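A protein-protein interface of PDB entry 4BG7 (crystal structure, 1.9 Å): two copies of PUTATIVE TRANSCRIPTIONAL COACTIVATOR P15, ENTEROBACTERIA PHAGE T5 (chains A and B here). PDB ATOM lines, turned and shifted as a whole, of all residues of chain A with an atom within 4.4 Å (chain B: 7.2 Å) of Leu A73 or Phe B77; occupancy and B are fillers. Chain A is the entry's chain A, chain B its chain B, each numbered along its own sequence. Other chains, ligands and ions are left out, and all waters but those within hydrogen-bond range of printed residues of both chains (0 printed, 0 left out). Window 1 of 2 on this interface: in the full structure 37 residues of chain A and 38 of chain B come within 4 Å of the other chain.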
ATOM      1  N   LEU A  30     -12.835  21.543  13.292  1.00  0.00           N
ATOM      2  CA  LEU A  30     -13.208  21.457  14.695  1.00  0.00           C
ATOM      3  C   LEU A  30     -14.510  22.176  14.878  1.00  0.00           C
ATOM      4  O   LEU A  30     -14.629  23.404  14.608  1.00  0.00           O
ATOM      5  CB  LEU A  30     -12.181  22.117  15.633  1.00  0.00           C
ATOM      6  CG  LEU A  30     -12.380  21.875  17.138  1.00  0.00           C
ATOM      7  CD1 LEU A  30     -12.271  20.390  17.376  1.00  0.00           C
ATOM      8  CD2 LEU A  30     -11.257  22.658  17.871  1.00  0.00           C
ATOM      9  N   MET A  41     -18.756  18.591  20.700  1.00  0.00           N
ATOM     10  CA  MET A  41     -17.550  18.982  19.977  1.00  0.00           C
ATOM     11  C   MET A  41     -16.998  17.807  19.215  1.00  0.00           C
ATOM     12  O   MET A  41     -17.006  16.678  19.672  1.00  0.00           O
ATOM     13  CB  MET A  41     -16.431  19.580  20.870  1.00  0.00           C
ATOM     14  CG  MET A  41     -16.027  18.764  22.058  1.00  0.00           C
ATOM     15  SD  MET A  41     -14.503  19.357  22.865  1.00  0.00           S
ATOM     16  CE  MET A  41     -14.647  18.423  24.362  1.00  0.00           C
ATOM     17  N   THR A  69     -15.798  17.781  29.864  1.00  0.00           N
ATOM     18  CA  THR A  69     -15.056  17.236  28.733  1.00  0.00           C
ATOM     19  C   THR A  69     -14.021  18.237  28.220  1.00  0.00           C
ATOM     20  O   THR A  69     -12.899  17.843  27.825  1.00  0.00           O
ATOM     21  CB  THR A  69     -15.965  16.746  27.583  1.00  0.00           C
ATOM     22  OG1 THR A  69     -16.710  17.862  27.098  1.00  0.00           O
ATOM     23  CG2 THR A  69     -16.915  15.652  28.059  1.00  0.00           C
ATOM     24  N   THR A  70     -14.371  19.503  28.195  1.00  0.00           N
ATOM     25  CA  THR A  70     -13.442  20.505  27.717  1.00  0.00           C
ATOM     26  C   THR A  70     -12.271  20.642  28.658  1.00  0.00           C
ATOM     27  O   THR A  70     -11.132  20.672  28.195  1.00  0.00           O
ATOM     28  CB  THR A  70     -14.117  21.820  27.436  1.00  0.00           C
ATOM     29  OG1 THR A  70     -14.790  22.305  28.610  1.00  0.00           O
ATOM     30  CG2 THR A  70     -15.126  21.704  26.243  1.00  0.00           C
ATOM     31  N   SER A  71     -12.539  20.692  29.982  1.00  0.00           N
ATOM     32  CA  SER A  71     -11.486  20.731  31.010  1.00  0.00           C
ATOM     33  C   SER A  71     -10.620  19.459  30.936  1.00  0.00           C
ATOM     34  O   SER A  71      -9.397  19.524  30.996  1.00  0.00           O
ATOM     35  CB  SER A  71     -12.103  20.855  32.407  1.00  0.00           C
ATOM     36  OG  SER A  71     -12.782  22.073  32.447  1.00  0.00           O
ATOM     37  N   GLN A  72     -11.233  18.308  30.736  1.00  0.00           N
ATOM     38  CA  GLN A  72     -10.406  17.076  30.614  1.00  0.00           C
ATOM     39  C   GLN A  72      -9.527  17.107  29.356  1.00  0.00           C
ATOM     40  O   GLN A  72      -8.405  16.660  29.352  1.00  0.00           O
ATOM     41  CB  GLN A  72     -11.280  15.873  30.584  1.00  0.00           C
ATOM     42  CG  GLN A  72     -10.575  14.524  30.470  1.00  0.00           C
ATOM     43  CD  GLN A  72      -9.611  14.236  31.619  1.00  0.00           C
ATOM     44  OE1 GLN A  72      -9.669  14.894  32.656  1.00  0.00           O
ATOM     45  NE2 GLN A  72      -8.746  13.206  31.451  1.00  0.00           N
ATOM     46  N   LEU A  73     -10.069  17.589  28.256  1.00  0.00           N
ATOM     47  CA  LEU A  73      -9.256  17.663  27.021  1.00  0.00           C
ATOM     48  C   LEU A  73      -8.101  18.660  27.181  1.00  0.00           C
ATOM     49  O   LEU A  73      -6.945  18.334  26.880  1.00  0.00           O
ATOM     50  CB  LEU A  73     -10.149  17.995  25.808  1.00  0.00           C
ATOM     51  CG  LEU A  73      -9.451  18.218  24.465  1.00  0.00           C
ATOM     52  CD1 LEU A  73      -8.512  17.055  24.119  1.00  0.00           C
ATOM     53  CD2 LEU A  73     -10.485  18.500  23.341  1.00  0.00           C
ATOM     54  N   PHE A  74      -8.389  19.823  27.732  1.00  0.00           N
ATOM     55  CA  PHE A  74      -7.389  20.891  27.945  1.00  0.00           C
ATOM     56  C   PHE A  74      -6.284  20.306  28.825  1.00  0.00           C
ATOM     57  O   PHE A  74      -5.076  20.378  28.513  1.00  0.00           O
ATOM     58  CB  PHE A  74      -8.006  22.132  28.635  1.00  0.00           C
ATOM     59  CG  PHE A  74      -7.151  23.373  28.584  1.00  0.00           C
ATOM     60  CD1 PHE A  74      -6.078  23.539  29.446  1.00  0.00           C
ATOM     61  CD2 PHE A  74      -7.430  24.394  27.664  1.00  0.00           C
ATOM     62  CE1 PHE A  74      -5.306  24.657  29.384  1.00  0.00           C
ATOM     63  CE2 PHE A  74      -6.635  25.551  27.580  1.00  0.00           C
ATOM     64  CZ  PHE A  74      -5.568  25.674  28.453  1.00  0.00           C
ATOM     65  N   TYR A  75      -6.715  19.650  29.890  1.00  0.00           N
ATOM     66  CA  TYR A  75      -5.747  18.964  30.779  1.00  0.00           C
ATOM     67  C   TYR A  75      -4.899  17.878  30.052  1.00  0.00           C
ATOM     68  O   TYR A  75      -3.591  17.854  30.161  1.00  0.00           O
ATOM     69  CB  TYR A  75      -6.466  18.435  32.019  1.00  0.00           C
ATOM     70  CG  TYR A  75      -5.755  17.307  32.712  1.00  0.00           C
ATOM     71  CD1 TYR A  75      -4.665  17.540  33.516  1.00  0.00           C
ATOM     72  CD2 TYR A  75      -6.078  15.996  32.418  1.00  0.00           C
ATOM     73  CE1 TYR A  75      -4.008  16.488  34.135  1.00  0.00           C
ATOM     74  CE2 TYR A  75      -5.448  14.961  33.009  1.00  0.00           C
ATOM     75  CZ  TYR A  75      -4.418  15.213  33.887  1.00  0.00           C
ATOM     76  OH  TYR A  75      -3.796  14.135  34.447  1.00  0.00           O
ATOM     77  N   ALA A  76      -5.591  16.968  29.346  1.00  0.00           N
ATOM     78  CA  ALA A  76      -4.903  15.788  28.749  1.00  0.00           C
ATOM     79  C   ALA A  76      -3.970  16.222  27.656  1.00  0.00           C
ATOM     80  O   ALA A  76      -2.790  15.719  27.587  1.00  0.00           O
ATOM     81  CB  ALA A  76      -5.881  14.680  28.228  1.00  0.00           C
ATOM     82  N   PHE A  77      -4.449  17.177  26.853  1.00  0.00           N
ATOM     83  CA  PHE A  77      -3.671  17.693  25.732  1.00  0.00           C
ATOM     84  C   PHE A  77      -2.443  18.501  26.211  1.00  0.00           C
ATOM     85  O   PHE A  77      -1.292  18.303  25.740  1.00  0.00           O
ATOM     86  CB  PHE A  77      -4.592  18.530  24.863  1.00  0.00           C
ATOM     87  CG  PHE A  77      -3.972  19.053  23.570  1.00  0.00           C
ATOM     88  CD1 PHE A  77      -3.177  18.279  22.789  1.00  0.00           C
ATOM     89  CD2 PHE A  77      -4.272  20.298  23.138  1.00  0.00           C
ATOM     90  CE1 PHE A  77      -2.662  18.761  21.601  1.00  0.00           C
ATOM     91  CE2 PHE A  77      -3.803  20.768  21.924  1.00  0.00           C
ATOM     92  CZ  PHE A  77      -2.972  20.002  21.183  1.00  0.00           C
ATOM     93  N   ILE B  19      -8.131   9.035  28.702  1.00  0.00           N
ATOM     94  CA  ILE B  19      -9.574   9.042  28.487  1.00  0.00           C
ATOM     95  C   ILE B  19     -10.134  10.465  28.585  1.00  0.00           C
ATOM     96  O   ILE B  19      -9.901  11.183  29.567  1.00  0.00           O
ATOM     97  CB  ILE B  19     -10.274   8.073  29.455  1.00  0.00           C
ATOM     98  CG1 ILE B  19      -9.789   6.638  29.166  1.00  0.00           C
ATOM     99  CG2 ILE B  19     -11.790   8.156  29.277  1.00  0.00           C
ATOM    100  CD1 ILE B  19      -9.732   5.641  30.334  1.00  0.00           C
ATOM    101  N   LEU B  20     -10.846  10.890  27.555  1.00  0.00           N
ATOM    102  CA  LEU B  20     -11.498  12.253  27.511  1.00  0.00           C
ATOM    103  C   LEU B  20     -12.934  12.205  27.995  1.00  0.00           C
ATOM    104  O   LEU B  20     -13.505  13.213  28.467  1.00  0.00           O
ATOM    105  CB  LEU B  20     -11.496  12.825  26.103  1.00  0.00           C
ATOM    106  CG  LEU B  20     -10.135  13.068  25.464  1.00  0.00           C
ATOM    107  CD1 LEU B  20     -10.271  13.776  24.132  1.00  0.00           C
ATOM    108  CD2 LEU B  20      -9.298  13.894  26.460  1.00  0.00           C
ATOM    109  N   LEU B  30      -7.615  10.318  23.857  1.00  0.00           N
ATOM    110  CA  LEU B  30      -6.593  11.117  23.252  1.00  0.00           C
ATOM    111  C   LEU B  30      -5.321  10.261  23.342  1.00  0.00           C
ATOM    112  O   LEU B  30      -4.988   9.794  24.428  1.00  0.00           O
ATOM    113  CB  LEU B  30      -6.345  12.384  24.024  1.00  0.00           C
ATOM    114  CG  LEU B  30      -5.219  13.306  23.497  1.00  0.00           C
ATOM    115  CD1 LEU B  30      -5.469  13.867  22.110  1.00  0.00           C
ATOM    116  CD2 LEU B  30      -5.161  14.463  24.485  1.00  0.00           C
ATOM    117  N   ILE B  43      -7.766  11.607  18.373  1.00  0.00           N
ATOM    118  CA  ILE B  43      -8.918  11.624  19.282  1.00  0.00           C
ATOM    119  C   ILE B  43      -9.883  10.658  18.601  1.00  0.00           C
ATOM    120  O   ILE B  43     -10.193  10.837  17.388  1.00  0.00           O
ATOM    121  CB  ILE B  43      -9.548  12.979  19.482  1.00  0.00           C
ATOM    122  CG1 ILE B  43      -8.598  13.900  20.257  1.00  0.00           C
ATOM    123  CG2 ILE B  43     -10.811  12.862  20.334  1.00  0.00           C
ATOM    124  CD1 ILE B  43      -9.083  15.358  20.211  1.00  0.00           C
ATOM    125  N   SER B  71      -0.223  22.735  17.312  1.00  0.00           N
ATOM    126  CA  SER B  71      -0.467  24.169  17.469  1.00  0.00           C
ATOM    127  C   SER B  71      -1.766  24.672  16.836  1.00  0.00           C
ATOM    128  O   SER B  71      -2.434  25.598  17.373  1.00  0.00           O
ATOM    129  CB  SER B  71       0.657  24.991  16.875  1.00  0.00           C
ATOM    130  OG  SER B  71       1.853  24.703  17.599  1.00  0.00           O
ATOM    131  N   GLN B  72      -2.049  24.078  15.675  1.00  0.00           N
ATOM    132  CA  GLN B  72      -3.293  24.315  14.969  1.00  0.00           C
ATOM    133  C   GLN B  72      -4.486  23.897  15.858  1.00  0.00           C
ATOM    134  O   GLN B  72      -5.418  24.669  16.042  1.00  0.00           O
ATOM    135  CB  GLN B  72      -3.274  23.537  13.645  1.00  0.00           C
ATOM    136  CG  GLN B  72      -4.439  23.841  12.715  1.00  0.00           C
ATOM    137  CD  GLN B  72      -4.516  25.291  12.295  1.00  0.00           C
ATOM    138  OE1 GLN B  72      -3.472  25.955  12.215  1.00  0.00           O
ATOM    139  NE2 GLN B  72      -5.758  25.806  12.032  1.00  0.00           N
ATOM    140  N   LEU B  73      -4.422  22.711  16.407  1.00  0.00           N
ATOM    141  CA  LEU B  73      -5.464  22.216  17.268  1.00  0.00           C
ATOM    142  C   LEU B  73      -5.607  23.022  18.547  1.00  0.00           C
ATOM    143  O   LEU B  73      -6.739  23.420  18.962  1.00  0.00           O
ATOM    144  CB  LEU B  73      -5.230  20.741  17.563  1.00  0.00           C
ATOM    145  CG  LEU B  73      -6.281  20.062  18.482  1.00  0.00           C
ATOM    146  CD1 LEU B  73      -7.718  20.176  17.916  1.00  0.00           C
ATOM    147  CD2 LEU B  73      -5.869  18.612  18.715  1.00  0.00           C
ATOM    148  N   PHE B  74      -4.477  23.341  19.179  1.00  0.00           N
ATOM    149  CA  PHE B  74      -4.539  24.212  20.371  1.00  0.00           C
ATOM    150  C   PHE B  74      -5.175  25.594  20.129  1.00  0.00           C
ATOM    151  O   PHE B  74      -5.959  26.089  20.911  1.00  0.00           O
ATOM    152  CB  PHE B  74      -3.137  24.348  21.084  1.00  0.00           C
ATOM    153  CG  PHE B  74      -3.232  24.883  22.508  1.00  0.00           C
ATOM    154  CD1 PHE B  74      -3.598  24.046  23.554  1.00  0.00           C
ATOM    155  CD2 PHE B  74      -2.970  26.212  22.805  1.00  0.00           C
ATOM    156  CE1 PHE B  74      -3.687  24.518  24.847  1.00  0.00           C
ATOM    157  CE2 PHE B  74      -3.045  26.683  24.106  1.00  0.00           C
ATOM    158  CZ  PHE B  74      -3.416  25.837  25.131  1.00  0.00           C
ATOM    159  N   TYR B  75      -4.797  26.243  19.051  1.00  0.00           N
ATOM    160  CA  TYR B  75      -5.408  27.487  18.637  1.00  0.00           C
ATOM    161  C   TYR B  75      -6.945  27.352  18.411  1.00  0.00           C
ATOM    162  O   TYR B  75      -7.725  28.170  18.851  1.00  0.00           O
ATOM    163  CB  TYR B  75      -4.746  27.927  17.304  1.00  0.00           C
ATOM    164  CG  TYR B  75      -5.657  28.730  16.433  1.00  0.00           C
ATOM    165  CD1 TYR B  75      -6.046  29.961  16.843  1.00  0.00           C
ATOM    166  CD2 TYR B  75      -6.178  28.217  15.204  1.00  0.00           C
ATOM    167  CE1 TYR B  75      -6.909  30.732  16.086  1.00  0.00           C
ATOM    168  CE2 TYR B  75      -7.058  29.000  14.442  1.00  0.00           C
ATOM    169  CZ  TYR B  75      -7.396  30.260  14.916  1.00  0.00           C
ATOM    170  OH  TYR B  75      -8.242  31.143  14.274  1.00  0.00           O
ATOM    171  N   ALA B  76      -7.343  26.282  17.748  1.00  0.00           N
ATOM    172  CA  ALA B  76      -8.770  26.176  17.329  1.00  0.00           C
ATOM    173  C   ALA B  76      -9.599  25.898  18.589  1.00  0.00           C
ATOM    174  O   ALA B  76     -10.600  26.568  18.824  1.00  0.00           O
ATOM    175  CB  ALA B  76      -8.900  25.099  16.300  1.00  0.00           C
ATOM    176  N   PHE B  77      -9.127  24.939  19.402  1.00  0.00           N
ATOM    177  CA  PHE B  77      -9.800  24.555  20.625  1.00  0.00           C
ATOM    178  C   PHE B  77      -9.938  25.773  21.541  1.00  0.00           C
ATOM    179  O   PHE B  77     -10.992  26.092  22.057  1.00  0.00           O
ATOM    180  CB  PHE B  77      -9.066  23.384  21.262  1.00  0.00           C
ATOM    181  CG  PHE B  77      -9.688  22.871  22.535  1.00  0.00           C
ATOM    182  CD1 PHE B  77     -11.087  22.660  22.621  1.00  0.00           C
ATOM    183  CD2 PHE B  77      -8.876  22.575  23.662  1.00  0.00           C
ATOM    184  CE1 PHE B  77     -11.656  22.181  23.800  1.00  0.00           C
ATOM    185  CE2 PHE B  77      -9.461  22.117  24.840  1.00  0.00           C
ATOM    186  CZ  PHE B  77     -10.854  21.913  24.902  1.00  0.00           C
ATOM    187  N   THR B  78      -8.838  26.486  21.753  1.00  0.00           N
ATOM    188  CA  THR B  78      -8.860  27.741  22.526  1.00  0.00           C
ATOM    189  C   THR B  78      -9.817  28.812  21.995  1.00  0.00           C
ATOM    190  O   THR B  78     -10.449  29.518  22.755  1.00  0.00           O
ATOM    191  CB  THR B  78      -7.407  28.358  22.522  1.00  0.00           C
ATOM    192  OG1 THR B  78      -6.559  27.481  23.288  1.00  0.00           O
ATOM    193  CG2 THR B  78      -7.418  29.709  23.060  1.00  0.00           C
ATOM    194  N   GLN B  79      -9.893  28.968  20.681  1.00  0.00           N
ATOM    195  CA  GLN B  79     -10.894  29.885  20.098  1.00  0.00           C
ATOM    196  C   GLN B  79     -12.359  29.516  20.439  1.00  0.00           C
ATOM    197  O   GLN B  79     -13.182  30.406  20.781  1.00  0.00           O
ATOM    198  CB  GLN B  79     -10.817  29.871  18.593  1.00  0.00           C
ATOM    199  CG  GLN B  79     -11.351  31.141  17.958  1.00  0.00           C
ATOM    200  CD  GLN B  79     -10.168  31.929  17.462  1.00  0.00           C
ATOM    201  OE1 GLN B  79      -9.316  32.388  18.269  1.00  0.00           O
ATOM    202  NE2 GLN B  79     -10.032  31.999  16.135  1.00  0.00           N
ATOM    203  N   ILE B  80     -12.677  28.213  20.307  1.00  0.00           N
ATOM    204  CA  ILE B  80     -14.055  27.777  20.576  1.00  0.00           C
ATOM    205  C   ILE B  80     -14.449  28.016  22.002  1.00  0.00           C
ATOM    206  O   ILE B  80     -15.525  28.552  22.266  1.00  0.00           O
ATOM    207  CB  ILE B  80     -14.436  26.336  20.041  1.00  0.00           C
ATOM    208  CG1 ILE B  80     -13.848  25.207  20.867  1.00  0.00           C
ATOM    209  CG2 ILE B  80     -14.111  26.135  18.526  1.00  0.00           C
ATOM    210  CD1 ILE B  80     -14.240  23.777  20.425  1.00  0.00           C
ATOM    211  N   LEU B  81     -13.538  27.728  22.929  1.00  0.00           N
ATOM    212  CA  LEU B  81     -13.766  28.001  24.323  1.00  0.00           C
ATOM    213  C   LEU B  81     -13.916  29.509  24.569  1.00  0.00           C
ATOM    214  O   LEU B  81     -14.763  29.920  25.334  1.00  0.00           O
ATOM    215  CB  LEU B  81     -12.621  27.430  25.192  1.00  0.00           C
ATOM    216  CG  LEU B  81     -12.370  25.943  25.179  1.00  0.00           C
ATOM    217  CD1 LEU B  81     -11.205  25.575  26.052  1.00  0.00           C
ATOM    218  CD2 LEU B  81     -13.649  25.180  25.625  1.00  0.00           C
ATOM    219  N   SER B  82     -13.108  30.331  23.909  1.00  0.00           N
ATOM    220  CA  SER B  82     -13.234  31.779  24.101  1.00  0.00           C
ATOM    221  C   SER B  82     -14.596  32.310  23.608  1.00  0.00           C
ATOM    222  O   SER B  82     -15.253  33.074  24.314  1.00  0.00           O
ATOM    223  CB  SER B  82     -12.110  32.543  23.388  1.00  0.00           C
ATOM    224  OG  SER B  82     -10.865  32.246  24.003  1.00  0.00           O
ATOM    225  N   GLU B  83     -15.005  31.885  22.404  1.00  0.00           N
ATOM    226  CA  GLU B  83     -16.326  32.268  21.837  1.00  0.00           C
ATOM    227  C   GLU B  83     -17.460  31.799  22.732  1.00  0.00           C
ATOM    228  O   GLU B  83     -18.461  32.484  22.935  1.00  0.00           O
ATOM    229  CB  GLU B  83     -16.498  31.666  20.464  1.00  0.00           C
ATOM    230  CG  GLU B  83     -17.675  32.250  19.683  1.00  0.00           C
ATOM    231  CD  GLU B  83     -17.500  33.734  19.439  1.00  0.00           C
ATOM    232  OE1 GLU B  83     -16.555  34.128  18.704  1.00  0.00           O
ATOM    233  OE2 GLU B  83     -18.288  34.501  20.029  1.00  0.00           O
ATOM    234  N   LEU B  87     -13.304  29.953  28.494  1.00  0.00           N
ATOM    235  CA  LEU B  87     -11.891  29.621  28.485  1.00  0.00           C
ATOM    236  C   LEU B  87     -11.273  29.618  29.913  1.00  0.00           C
ATOM    237  O   LEU B  87     -10.604  28.686  30.297  1.00  0.00           O
ATOM    238  CB  LEU B  87     -11.123  30.580  27.610  1.00  0.00           C
ATOM    239  CG  LEU B  87      -9.635  30.289  27.452  1.00  0.00           C
ATOM    240  CD1 LEU B  87      -9.334  28.838  27.096  1.00  0.00           C
ATOM    241  CD2 LEU B  87      -9.135  31.230  26.389  1.00  0.00           C
ATOM    242  N   VAL B  90     -12.451  26.735  32.128  1.00  0.00           N
ATOM    243  CA  VAL B  90     -11.844  25.481  31.709  1.00  0.00           C
ATOM    244  C   VAL B  90     -10.391  25.475  32.147  1.00  0.00           C
ATOM    245  O   VAL B  90      -9.876  24.420  32.536  1.00  0.00           O
ATOM    246  CB  VAL B  90     -11.935  25.290  30.180  1.00  0.00           C
ATOM    247  CG1 VAL B  90     -11.107  24.075  29.702  1.00  0.00           C
ATOM    248  CG2 VAL B  90     -13.424  25.205  29.784  1.00  0.00           C
ATOM    249  N   ALA B  94      -8.905  22.644  34.483  1.00  0.00           N
ATOM    250  CA  ALA B  94      -7.791  21.814  34.023  1.00  0.00           C
ATOM    251  C   ALA B  94      -6.622  21.875  35.005  1.00  0.00           C
ATOM    252  O   ALA B  94      -5.981  20.874  35.264  1.00  0.00           O
ATOM    253  CB  ALA B  94      -7.339  22.258  32.644  1.00  0.00           C
ATOM    254  N   LEU B  97      -7.320  19.623  37.784  1.00  0.00           N
ATOM    255  CA  LEU B  97      -7.177  18.206  37.451  1.00  0.00           C
ATOM    256  C   LEU B  97      -5.730  17.731  37.554  1.00  0.00           C
ATOM    257  O   LEU B  97      -5.463  16.543  37.782  1.00  0.00           O
ATOM    258  CB  LEU B  97      -7.717  17.975  36.021  1.00  0.00           C
ATOM    259  CG  LEU B  97      -9.217  18.163  35.796  1.00  0.00           C
ATOM    260  CD1 LEU B  97      -9.524  17.940  34.313  1.00  0.00           C
ATOM    261  CD2 LEU B  97      -9.971  17.198  36.690  1.00  0.00           C
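NE2 of Gln A72 lies within hydrogen-bond range of O of Ile B19 (3.0 Å).
OG1 of Thr B78 is in hydrogen-bond range of O of Phe B74, at 2.8 Å.
O of Leu B81 sits at hydrogen-bond distance from N of Leu B87 (3.5 Å).
C of Ala B76 touches CD2 of Leu A30, 3.7 Å away.
CG2 of Val B90 touches OG1 of Thr A70, 3.4 Å away.
Leu B20 touches Leu A73.
CD2 of Leu A73 touches CZ of Phe B77 (3.8 Å).
Phe A74 touches Phe B74.
Val B90 touches Phe A74.
Ala B94 touches Phe A74.
CB of Ala A76 touches CD2 of Leu B20 (3.9 Å).
Leu B30 touches Ala A76.
Leu B30 touches Phe A77 (CD2 to N, 3.7 Å).
Of the printed residues of chain B, Leu A30 touches Ala B76 and Phe B77.
Printed residues of chain B within 4 Å of Thr A70: Phe B77, Leu B81 and Val B90.
Printed residues of chain B within 4 Å of Gln A72: Ile B19 (3.0 Å), Leu B20 (3.8 Å) and Leu B97 (3.5 Å).
Printed residues of chain A within 4 Å of Ala B76: Leu A30.
Of the printed residues of chain A, Phe B77 touches Leu A30, Thr A70, Leu A73 and Phe A74.
Ser B82 touches none of the printed residues of chain A.
Of the 21 printed residues of chain B, 10 touch a printed residue of chain A.
Hydrophobic or aromatic side chains of chain B within 4 Å of the printed part of chain A: Leu B20, Leu B30, Phe B74, Ala B76, Phe B77, Leu B81, Val B90, Ala B94 and Leu B97.
Hydrophobic or aromatic side chains of chain A that line the printed part of chain B: Leu A30, Leu A73, Phe A74, Tyr A75, Ala A76 and Phe A77.
Among the printed residues, no Asp or Glu carboxylate lies within 4 Å of a Lys or Arg side-chain nitrogen of the other chain.
Leu A30 touches Ala B76, and with the chains exchanged Ala A76 touches Leu B30.
Leu A30 touches Phe B77, and with the chains exchanged Phe A77 touches Leu B30.
Leu A73 touches Phe B77, but with the chains exchanged Phe A77 does not touch Leu B73 (4.1 Å).
Phe A74 touches Phe B77, and with the chains exchanged Phe A77 touches Phe B74.
Of the 23 pairs that touch across the chains among the printed residues, 7 have their exchanged pair printed and touching as well.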
